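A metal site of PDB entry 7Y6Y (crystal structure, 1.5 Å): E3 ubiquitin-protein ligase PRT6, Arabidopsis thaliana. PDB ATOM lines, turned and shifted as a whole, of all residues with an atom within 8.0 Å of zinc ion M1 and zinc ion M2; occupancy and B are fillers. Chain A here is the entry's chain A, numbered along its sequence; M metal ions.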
ATOM      1  N   VAL A   8      21.645 -27.301 -26.392  1.00  0.00           N
ATOM      2  CA  VAL A   8      21.767 -27.131 -24.934  1.00  0.00           C
ATOM      3  C   VAL A   8      23.177 -27.527 -24.468  1.00  0.00           C
ATOM      4  O   VAL A   8      23.735 -28.498 -24.944  1.00  0.00           O
ATOM      5  CB  VAL A   8      20.722 -27.936 -24.172  1.00  0.00           C
ATOM      6  CG1 VAL A   8      21.064 -27.988 -22.677  1.00  0.00           C
ATOM      7  CG2 VAL A   8      19.331 -27.333 -24.349  1.00  0.00           C
ATOM      8  N   CYS A   9      23.733 -26.749 -23.543  1.00  0.00           N
ATOM      9  CA  CYS A   9      25.074 -27.005 -23.048  1.00  0.00           C
ATOM     10  C   CYS A   9      25.169 -28.359 -22.344  1.00  0.00           C
ATOM     11  O   CYS A   9      25.996 -29.201 -22.687  1.00  0.00           O
ATOM     12  CB  CYS A   9      25.484 -25.903 -22.064  1.00  0.00           C
ATOM     13  SG  CYS A   9      27.164 -26.177 -21.306  1.00  0.00           S
ATOM     14  N   GLY A  10      24.403 -28.514 -21.272  1.00  0.00           N
ATOM     15  CA  GLY A  10      24.291 -29.769 -20.543  1.00  0.00           C
ATOM     16  C   GLY A  10      25.585 -30.231 -19.858  1.00  0.00           C
ATOM     17  O   GLY A  10      25.648 -31.378 -19.402  1.00  0.00           O
ATOM     18  N   SER A  11      26.616 -29.382 -19.804  1.00  0.00           N
ATOM     19  CA  SER A  11      27.817 -29.698 -19.027  1.00  0.00           C
ATOM     20  C   SER A  11      27.451 -30.057 -17.587  1.00  0.00           C
ATOM     21  O   SER A  11      26.580 -29.446 -16.985  1.00  0.00           O
ATOM     22  CB  SER A  11      28.726 -28.487 -18.988  1.00  0.00           C
ATOM     23  OG  SER A  11      29.812 -28.652 -18.109  1.00  0.00           O
ATOM     24  N   VAL A  12      28.226 -30.971 -17.004  1.00  0.00           N
ATOM     25  CA  VAL A  12      27.866 -31.610 -15.727  1.00  0.00           C
ATOM     26  C   VAL A  12      28.841 -31.192 -14.637  1.00  0.00           C
ATOM     27  O   VAL A  12      30.062 -31.145 -14.841  1.00  0.00           O
ATOM     28  CB  VAL A  12      27.792 -33.147 -15.840  1.00  0.00           C
ATOM     29  CG1 VAL A  12      27.755 -33.780 -14.436  1.00  0.00           C
ATOM     30  CG2 VAL A  12      26.588 -33.572 -16.643  1.00  0.00           C
ATOM     31  N   TRP A  13      28.284 -30.901 -13.456  1.00  0.00           N
ATOM     32  CA  TRP A  13      29.061 -30.550 -12.282  1.00  0.00           C
ATOM     33  C   TRP A  13      29.100 -31.718 -11.325  1.00  0.00           C
ATOM     34  O   TRP A  13      28.148 -32.490 -11.191  1.00  0.00           O
ATOM     35  CB  TRP A  13      28.491 -29.335 -11.536  1.00  0.00           C
ATOM     36  CG  TRP A  13      28.356 -28.155 -12.390  1.00  0.00           C
ATOM     37  CD1 TRP A  13      29.338 -27.518 -13.069  1.00  0.00           C
ATOM     38  CD2 TRP A  13      27.137 -27.474 -12.701  1.00  0.00           C
ATOM     39  NE1 TRP A  13      28.812 -26.483 -13.806  1.00  0.00           N
ATOM     40  CE2 TRP A  13      27.460 -26.432 -13.587  1.00  0.00           C
ATOM     41  CE3 TRP A  13      25.810 -27.655 -12.323  1.00  0.00           C
ATOM     42  CZ2 TRP A  13      26.496 -25.562 -14.097  1.00  0.00           C
ATOM     43  CZ3 TRP A  13      24.850 -26.792 -12.829  1.00  0.00           C
ATOM     44  CH2 TRP A  13      25.200 -25.758 -13.710  1.00  0.00           C
ATOM     45  N   ALA A  32      20.866 -23.030 -13.070  1.00  0.00           N
ATOM     46  CA  ALA A  32      22.239 -22.535 -13.001  1.00  0.00           C
ATOM     47  C   ALA A  32      22.950 -22.746 -14.340  1.00  0.00           C
ATOM     48  O   ALA A  32      22.563 -23.580 -15.165  1.00  0.00           O
ATOM     49  CB  ALA A  32      23.027 -23.215 -11.875  1.00  0.00           C
ATOM     50  N   ILE A  33      24.002 -21.976 -14.537  1.00  0.00           N
ATOM     51  CA  ILE A  33      24.790 -22.104 -15.748  1.00  0.00           C
ATOM     52  C   ILE A  33      26.259 -22.205 -15.381  1.00  0.00           C
ATOM     53  O   ILE A  33      26.734 -21.657 -14.379  1.00  0.00           O
ATOM     54  CB  ILE A  33      24.561 -20.988 -16.773  1.00  0.00           C
ATOM     55  CG1 ILE A  33      24.907 -19.601 -16.244  1.00  0.00           C
ATOM     56  CG2 ILE A  33      23.097 -21.080 -17.279  1.00  0.00           C
ATOM     57  CD1 ILE A  33      24.875 -18.621 -17.432  1.00  0.00           C
ATOM     58  N   CYS A  34      26.998 -22.903 -16.233  1.00  0.00           N
ATOM     59  CA  CYS A  34      28.421 -23.117 -16.014  1.00  0.00           C
ATOM     60  C   CYS A  34      29.187 -21.813 -16.203  1.00  0.00           C
ATOM     61  O   CYS A  34      28.708 -20.845 -16.804  1.00  0.00           O
ATOM     62  CB  CYS A  34      28.981 -24.215 -16.940  1.00  0.00           C
ATOM     63  SG  CYS A  34      29.077 -23.850 -18.714  1.00  0.00           S
ATOM     64  N   VAL A  35      30.401 -21.794 -15.668  1.00  0.00           N
ATOM     65  CA  VAL A  35      31.205 -20.591 -15.728  1.00  0.00           C
ATOM     66  C   VAL A  35      31.503 -20.179 -17.162  1.00  0.00           C
ATOM     67  O   VAL A  35      31.356 -18.987 -17.487  1.00  0.00           O
ATOM     68  CB  VAL A  35      32.484 -20.757 -14.888  1.00  0.00           C
ATOM     69  CG1 VAL A  35      33.430 -19.559 -15.088  1.00  0.00           C
ATOM     70  CG2 VAL A  35      32.138 -20.923 -13.410  1.00  0.00           C
ATOM     71  N   PRO A  36      31.896 -21.078 -18.080  1.00  0.00           N
ATOM     72  CA  PRO A  36      32.108 -20.627 -19.469  1.00  0.00           C
ATOM     73  C   PRO A  36      30.867 -20.012 -20.105  1.00  0.00           C
ATOM     74  O   PRO A  36      30.962 -19.010 -20.821  1.00  0.00           O
ATOM     75  CB  PRO A  36      32.535 -21.911 -20.196  1.00  0.00           C
ATOM     76  CG  PRO A  36      33.067 -22.820 -19.142  1.00  0.00           C
ATOM     77  CD  PRO A  36      32.307 -22.490 -17.886  1.00  0.00           C
ATOM     78  N   CYS A  37      29.711 -20.614 -19.882  1.00  0.00           N
ATOM     79  CA  CYS A  37      28.467 -20.049 -20.417  1.00  0.00           C
ATOM     80  C   CYS A  37      28.195 -18.675 -19.830  1.00  0.00           C
ATOM     81  O   CYS A  37      27.781 -17.757 -20.551  1.00  0.00           O
ATOM     82  CB  CYS A  37      27.317 -21.008 -20.140  1.00  0.00           C
ATOM     83  SG  CYS A  37      27.371 -22.423 -21.359  1.00  0.00           S
ATOM     84  N   PHE A  38      28.424 -18.510 -18.523  1.00  0.00           N
ATOM     85  CA  PHE A  38      28.241 -17.201 -17.913  1.00  0.00           C
ATOM     86  C   PHE A  38      29.153 -16.170 -18.555  1.00  0.00           C
ATOM     87  O   PHE A  38      28.738 -15.053 -18.883  1.00  0.00           O
ATOM     88  CB  PHE A  38      28.494 -17.264 -16.392  1.00  0.00           C
ATOM     89  CG  PHE A  38      28.287 -15.944 -15.710  1.00  0.00           C
ATOM     90  CD1 PHE A  38      27.032 -15.559 -15.308  1.00  0.00           C
ATOM     91  CD2 PHE A  38      29.355 -15.085 -15.505  1.00  0.00           C
ATOM     92  CE1 PHE A  38      26.836 -14.315 -14.689  1.00  0.00           C
ATOM     93  CE2 PHE A  38      29.191 -13.861 -14.886  1.00  0.00           C
ATOM     94  CZ  PHE A  38      27.914 -13.481 -14.493  1.00  0.00           C
ATOM     95  N   ASN A  40      30.449 -16.066 -21.462  1.00  0.00           N
ATOM     96  CA  ASN A  40      30.193 -15.794 -22.864  1.00  0.00           C
ATOM     97  C   ASN A  40      28.772 -15.271 -23.091  1.00  0.00           C
ATOM     98  O   ASN A  40      28.310 -15.263 -24.223  1.00  0.00           O
ATOM     99  CB  ASN A  40      30.474 -17.030 -23.707  1.00  0.00           C
ATOM    100  CG  ASN A  40      31.956 -17.275 -23.884  1.00  0.00           C
ATOM    101  OD1 ASN A  40      32.553 -18.062 -23.178  1.00  0.00           O
ATOM    102  ND2 ASN A  40      32.559 -16.585 -24.834  1.00  0.00           N
ATOM    103  N   GLY A  41      28.084 -14.838 -22.029  1.00  0.00           N
ATOM    104  CA  GLY A  41      26.794 -14.183 -22.140  1.00  0.00           C
ATOM    105  C   GLY A  41      26.831 -12.779 -21.560  1.00  0.00           C
ATOM    106  O   GLY A  41      27.902 -12.287 -21.218  1.00  0.00           O
ATOM    107  N   CYS A  57      23.555 -29.927 -13.869  1.00  0.00           N
ATOM    108  CA  CYS A  57      23.969 -29.667 -15.236  1.00  0.00           C
ATOM    109  C   CYS A  57      23.590 -28.255 -15.664  1.00  0.00           C
ATOM    110  O   CYS A  57      22.649 -27.647 -15.140  1.00  0.00           O
ATOM    111  CB  CYS A  57      23.407 -30.720 -16.203  1.00  0.00           C
ATOM    112  SG  CYS A  57      21.616 -30.758 -16.319  1.00  0.00           S
ATOM    113  N   CYS A  58      24.361 -27.745 -16.632  1.00  0.00           N
ATOM    114  CA  CYS A  58      24.197 -26.378 -17.088  1.00  0.00           C
ATOM    115  C   CYS A  58      22.918 -26.203 -17.910  1.00  0.00           C
ATOM    116  O   CYS A  58      22.630 -26.995 -18.810  1.00  0.00           O
ATOM    117  CB  CYS A  58      25.409 -25.975 -17.937  1.00  0.00           C
ATOM    118  SG  CYS A  58      25.262 -24.351 -18.620  1.00  0.00           S
ATOM    119  N   ASP A  59      22.171 -25.146 -17.626  1.00  0.00           N
ATOM    120  CA  ASP A  59      20.874 -24.899 -18.261  1.00  0.00           C
ATOM    121  C   ASP A  59      20.964 -24.019 -19.507  1.00  0.00           C
ATOM    122  O   ASP A  59      19.920 -23.709 -20.122  1.00  0.00           O
ATOM    123  CB  ASP A  59      19.938 -24.236 -17.240  1.00  0.00           C
ATOM    124  CG  ASP A  59      19.512 -25.197 -16.129  1.00  0.00           C
ATOM    125  OD1 ASP A  59      19.182 -26.363 -16.465  1.00  0.00           O
ATOM    126  OD2 ASP A  59      19.563 -24.816 -14.944  1.00  0.00           O
ATOM    127  N   CYS A  60      22.160 -23.598 -19.885  1.00  0.00           N
ATOM    128  CA  CYS A  60      22.317 -22.617 -20.957  1.00  0.00           C
ATOM    129  C   CYS A  60      21.862 -23.241 -22.256  1.00  0.00           C
ATOM    130  O   CYS A  60      22.248 -24.374 -22.568  1.00  0.00           O
ATOM    131  CB  CYS A  60      23.776 -22.198 -21.082  1.00  0.00           C
ATOM    132  SG  CYS A  60      24.025 -20.933 -22.336  1.00  0.00           S
ATOM    133  N   GLY A  61      21.007 -22.538 -22.993  1.00  0.00           N
ATOM    134  CA  GLY A  61      20.416 -23.054 -24.226  1.00  0.00           C
ATOM    135  C   GLY A  61      19.066 -23.720 -24.065  1.00  0.00           C
ATOM    136  O   GLY A  61      18.397 -23.967 -25.076  1.00  0.00           O
ATOM    137  N   ASP A  62      18.623 -23.978 -22.834  1.00  0.00           N
ATOM    138  CA  ASP A  62      17.350 -24.640 -22.551  1.00  0.00           C
ATOM    139  C   ASP A  62      16.323 -23.606 -22.106  1.00  0.00           C
ATOM    140  O   ASP A  62      16.303 -23.203 -20.944  1.00  0.00           O
ATOM    141  CB  ASP A  62      17.570 -25.713 -21.480  1.00  0.00           C
ATOM    142  CG  ASP A  62      16.280 -26.427 -21.060  1.00  0.00           C
ATOM    143  OD1 ASP A  62      15.211 -26.186 -21.686  1.00  0.00           O
ATOM    144  OD2 ASP A  62      16.353 -27.247 -20.095  1.00  0.00           O
ATOM    145  N   TRP A  66      16.015 -21.511 -18.530  1.00  0.00           N
ATOM    146  CA  TRP A  66      16.787 -20.274 -18.563  1.00  0.00           C
ATOM    147  C   TRP A  66      16.211 -19.350 -19.637  1.00  0.00           C
ATOM    148  O   TRP A  66      15.826 -19.814 -20.722  1.00  0.00           O
ATOM    149  CB  TRP A  66      18.240 -20.654 -18.852  1.00  0.00           C
ATOM    150  CG  TRP A  66      19.300 -19.674 -18.472  1.00  0.00           C
ATOM    151  CD1 TRP A  66      19.912 -18.774 -19.290  1.00  0.00           C
ATOM    152  CD2 TRP A  66      19.869 -19.503 -17.180  1.00  0.00           C
ATOM    153  NE1 TRP A  66      20.849 -18.044 -18.579  1.00  0.00           N
ATOM    154  CE2 TRP A  66      20.831 -18.493 -17.275  1.00  0.00           C
ATOM    155  CE3 TRP A  66      19.675 -20.135 -15.947  1.00  0.00           C
ATOM    156  CZ2 TRP A  66      21.600 -18.088 -16.184  1.00  0.00           C
ATOM    157  CZ3 TRP A  66      20.373 -19.736 -14.888  1.00  0.00           C
ATOM    158  CH2 TRP A  66      21.344 -18.726 -14.994  1.00  0.00           C
ATOM    159  N   GLY A  70      19.557 -14.724 -21.668  1.00  0.00           N
ATOM    160  CA  GLY A  70      20.655 -15.152 -20.826  1.00  0.00           C
ATOM    161  C   GLY A  70      21.506 -16.248 -21.400  1.00  0.00           C
ATOM    162  O   GLY A  70      22.456 -16.700 -20.740  1.00  0.00           O
ATOM    163  N   PHE A  71      21.219 -16.693 -22.627  1.00  0.00           N
ATOM    164  CA  PHE A  71      22.045 -17.699 -23.292  1.00  0.00           C
ATOM    165  C   PHE A  71      23.380 -17.112 -23.715  1.00  0.00           C
ATOM    166  O   PHE A  71      23.496 -15.921 -24.010  1.00  0.00           O
ATOM    167  CB  PHE A  71      21.366 -18.224 -24.545  1.00  0.00           C
ATOM    168  CG  PHE A  71      20.130 -19.038 -24.308  1.00  0.00           C
ATOM    169  CD1 PHE A  71      19.348 -19.415 -25.403  1.00  0.00           C
ATOM    170  CD2 PHE A  71      19.715 -19.413 -23.041  1.00  0.00           C
ATOM    171  CE1 PHE A  71      18.199 -20.183 -25.243  1.00  0.00           C
ATOM    172  CE2 PHE A  71      18.575 -20.197 -22.873  1.00  0.00           C
ATOM    173  CZ  PHE A  71      17.815 -20.573 -23.967  1.00  0.00           C
ATOM    174  N   CYS A  72      24.379 -17.954 -23.753  1.00  0.00           N
ATOM    175  CA  CYS A  72      25.702 -17.536 -24.227  1.00  0.00           C
ATOM    176  C   CYS A  72      25.755 -17.626 -25.743  1.00  0.00           C
ATOM    177  O   CYS A  72      24.888 -18.187 -26.392  1.00  0.00           O
ATOM    178  CB  CYS A  72      26.803 -18.389 -23.610  1.00  0.00           C
ATOM    179  SG  CYS A  72      27.130 -19.975 -24.403  1.00  0.00           S
ATOM    180  N   SER A  73      26.856 -17.123 -26.298  1.00  0.00           N
ATOM    181  CA  SER A  73      26.992 -17.022 -27.750  1.00  0.00           C
ATOM    182  C   SER A  73      27.105 -18.384 -28.435  1.00  0.00           C
ATOM    183  O   SER A  73      26.936 -18.452 -29.667  1.00  0.00           O
ATOM    184  CB  SER A  73      28.224 -16.167 -28.074  1.00  0.00           C
ATOM    185  OG  SER A  73      29.381 -16.705 -27.466  1.00  0.00           O
ATOM    186  N   ASN A  74      27.363 -19.446 -27.704  1.00  0.00           N
ATOM    187  CA  ASN A  74      27.509 -20.773 -28.260  1.00  0.00           C
ATOM    188  C   ASN A  74      26.242 -21.615 -28.190  1.00  0.00           C
ATOM    189  O   ASN A  74      26.199 -22.681 -28.814  1.00  0.00           O
ATOM    190  CB  ASN A  74      28.642 -21.537 -27.553  1.00  0.00           C
ATOM    191  CG  ASN A  74      29.995 -20.931 -27.784  1.00  0.00           C
ATOM    192  OD1 ASN A  74      30.814 -20.854 -26.853  1.00  0.00           O
ATOM    193  ND2 ASN A  74      30.252 -20.481 -29.004  1.00  0.00           N
ATOM    194  N   HIS A  75      25.199 -21.152 -27.497  1.00  0.00           N
ATOM    195  CA  HIS A  75      23.996 -21.960 -27.307  1.00  0.00           C
ATOM    196  C   HIS A  75      22.733 -21.180 -27.669  1.00  0.00           C
ATOM    197  O   HIS A  75      21.661 -21.392 -27.090  1.00  0.00           O
ATOM    198  CB  HIS A  75      23.935 -22.473 -25.862  1.00  0.00           C
ATOM    199  CG  HIS A  75      25.091 -23.349 -25.522  1.00  0.00           C
ATOM    200  ND1 HIS A  75      26.029 -23.030 -24.563  1.00  0.00           N
ATOM    201  CD2 HIS A  75      25.527 -24.508 -26.088  1.00  0.00           C
ATOM    202  CE1 HIS A  75      26.969 -23.955 -24.528  1.00  0.00           C
ATOM    203  NE2 HIS A  75      26.686 -24.866 -25.446  1.00  0.00           N
ATOM    204  N   LYS A  76      22.823 -20.319 -28.683  1.00  0.00           N
ATOM    205  CA  LYS A  76      21.666 -19.579 -29.167  1.00  0.00           C
ATOM    206  C   LYS A  76      21.145 -20.219 -30.448  1.00  0.00           C
ATOM    207  O   LYS A  76      20.020 -19.929 -30.843  1.00  0.00           O
ATOM    208  CB  LYS A  76      22.021 -18.133 -29.415  1.00  0.00           C
ATOM    209  CG  LYS A  76      22.243 -17.336 -28.163  1.00  0.00           C
ATOM    210  CD  LYS A  76      22.413 -15.883 -28.541  1.00  0.00           C
ATOM    211  CE  LYS A  76      23.019 -15.130 -27.425  1.00  0.00           C
ATOM    212  NZ  LYS A  76      22.898 -13.668 -27.615  1.00  0.00           N
HETATM  213 ZN    ZN M   1      26.003 -21.605 -23.181  1.00  0.00          ZN
HETATM  214 ZN    ZN M   2      27.175 -24.302 -19.945  1.00  0.00          ZN
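The backbone carbonyl oxygen (O) of Cys 60 sits at hydrogen-bond distance from the backbone NH (N) of Cys 9, 3.0 Å away.
The backbone NH (N) of Cys 60 sits close to the side-chain sulfur (SG) of Cys 58 (3.4 Å).
The side-chain sulfur of Cys 9 lies close to the backbone NH of Ser 11 (3.6 Å).
N of Cys 58 is in hydrogen-bond range of O of Ser 11 (2.8 Å).
The backbone NH of Gly 10 is in hydrogen-bond range of the backbone carbonyl oxygen of Cys 58, 3.4 Å away.
SG of Cys 72 sits close to N of Asn 74, 3.4 Å away.
The nearest printed residue that does not touch zinc ion M1 is Cys 9 (4.5 Å).
Along chain A the residues within 4 Å of zinc ion M2 span positions 9 to 58.
Zinc ion M1 is bound by ND1 of His 75 (2.0 Å).
The side-chain sulfur (SG) of Cys 60 is bound to zinc ion M1 (2.3 Å).
SG of Cys 72 binds zinc ion M1 (2.3 Å).
SG of Cys 37 binds zinc ion M1 (2.4 Å).
SG of Cys 34 binds zinc ion M2 (2.3 Å).
Zinc ion M2 is bound by the side-chain sulfur (SG) of Cys 9.
SG of Cys 58 is bound to zinc ion M2 (2.3 Å).
SG of Cys 37 is bound to zinc ion M2, 2.4 Å away.
Zinc ion M2 has four donor atoms within binding distance.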
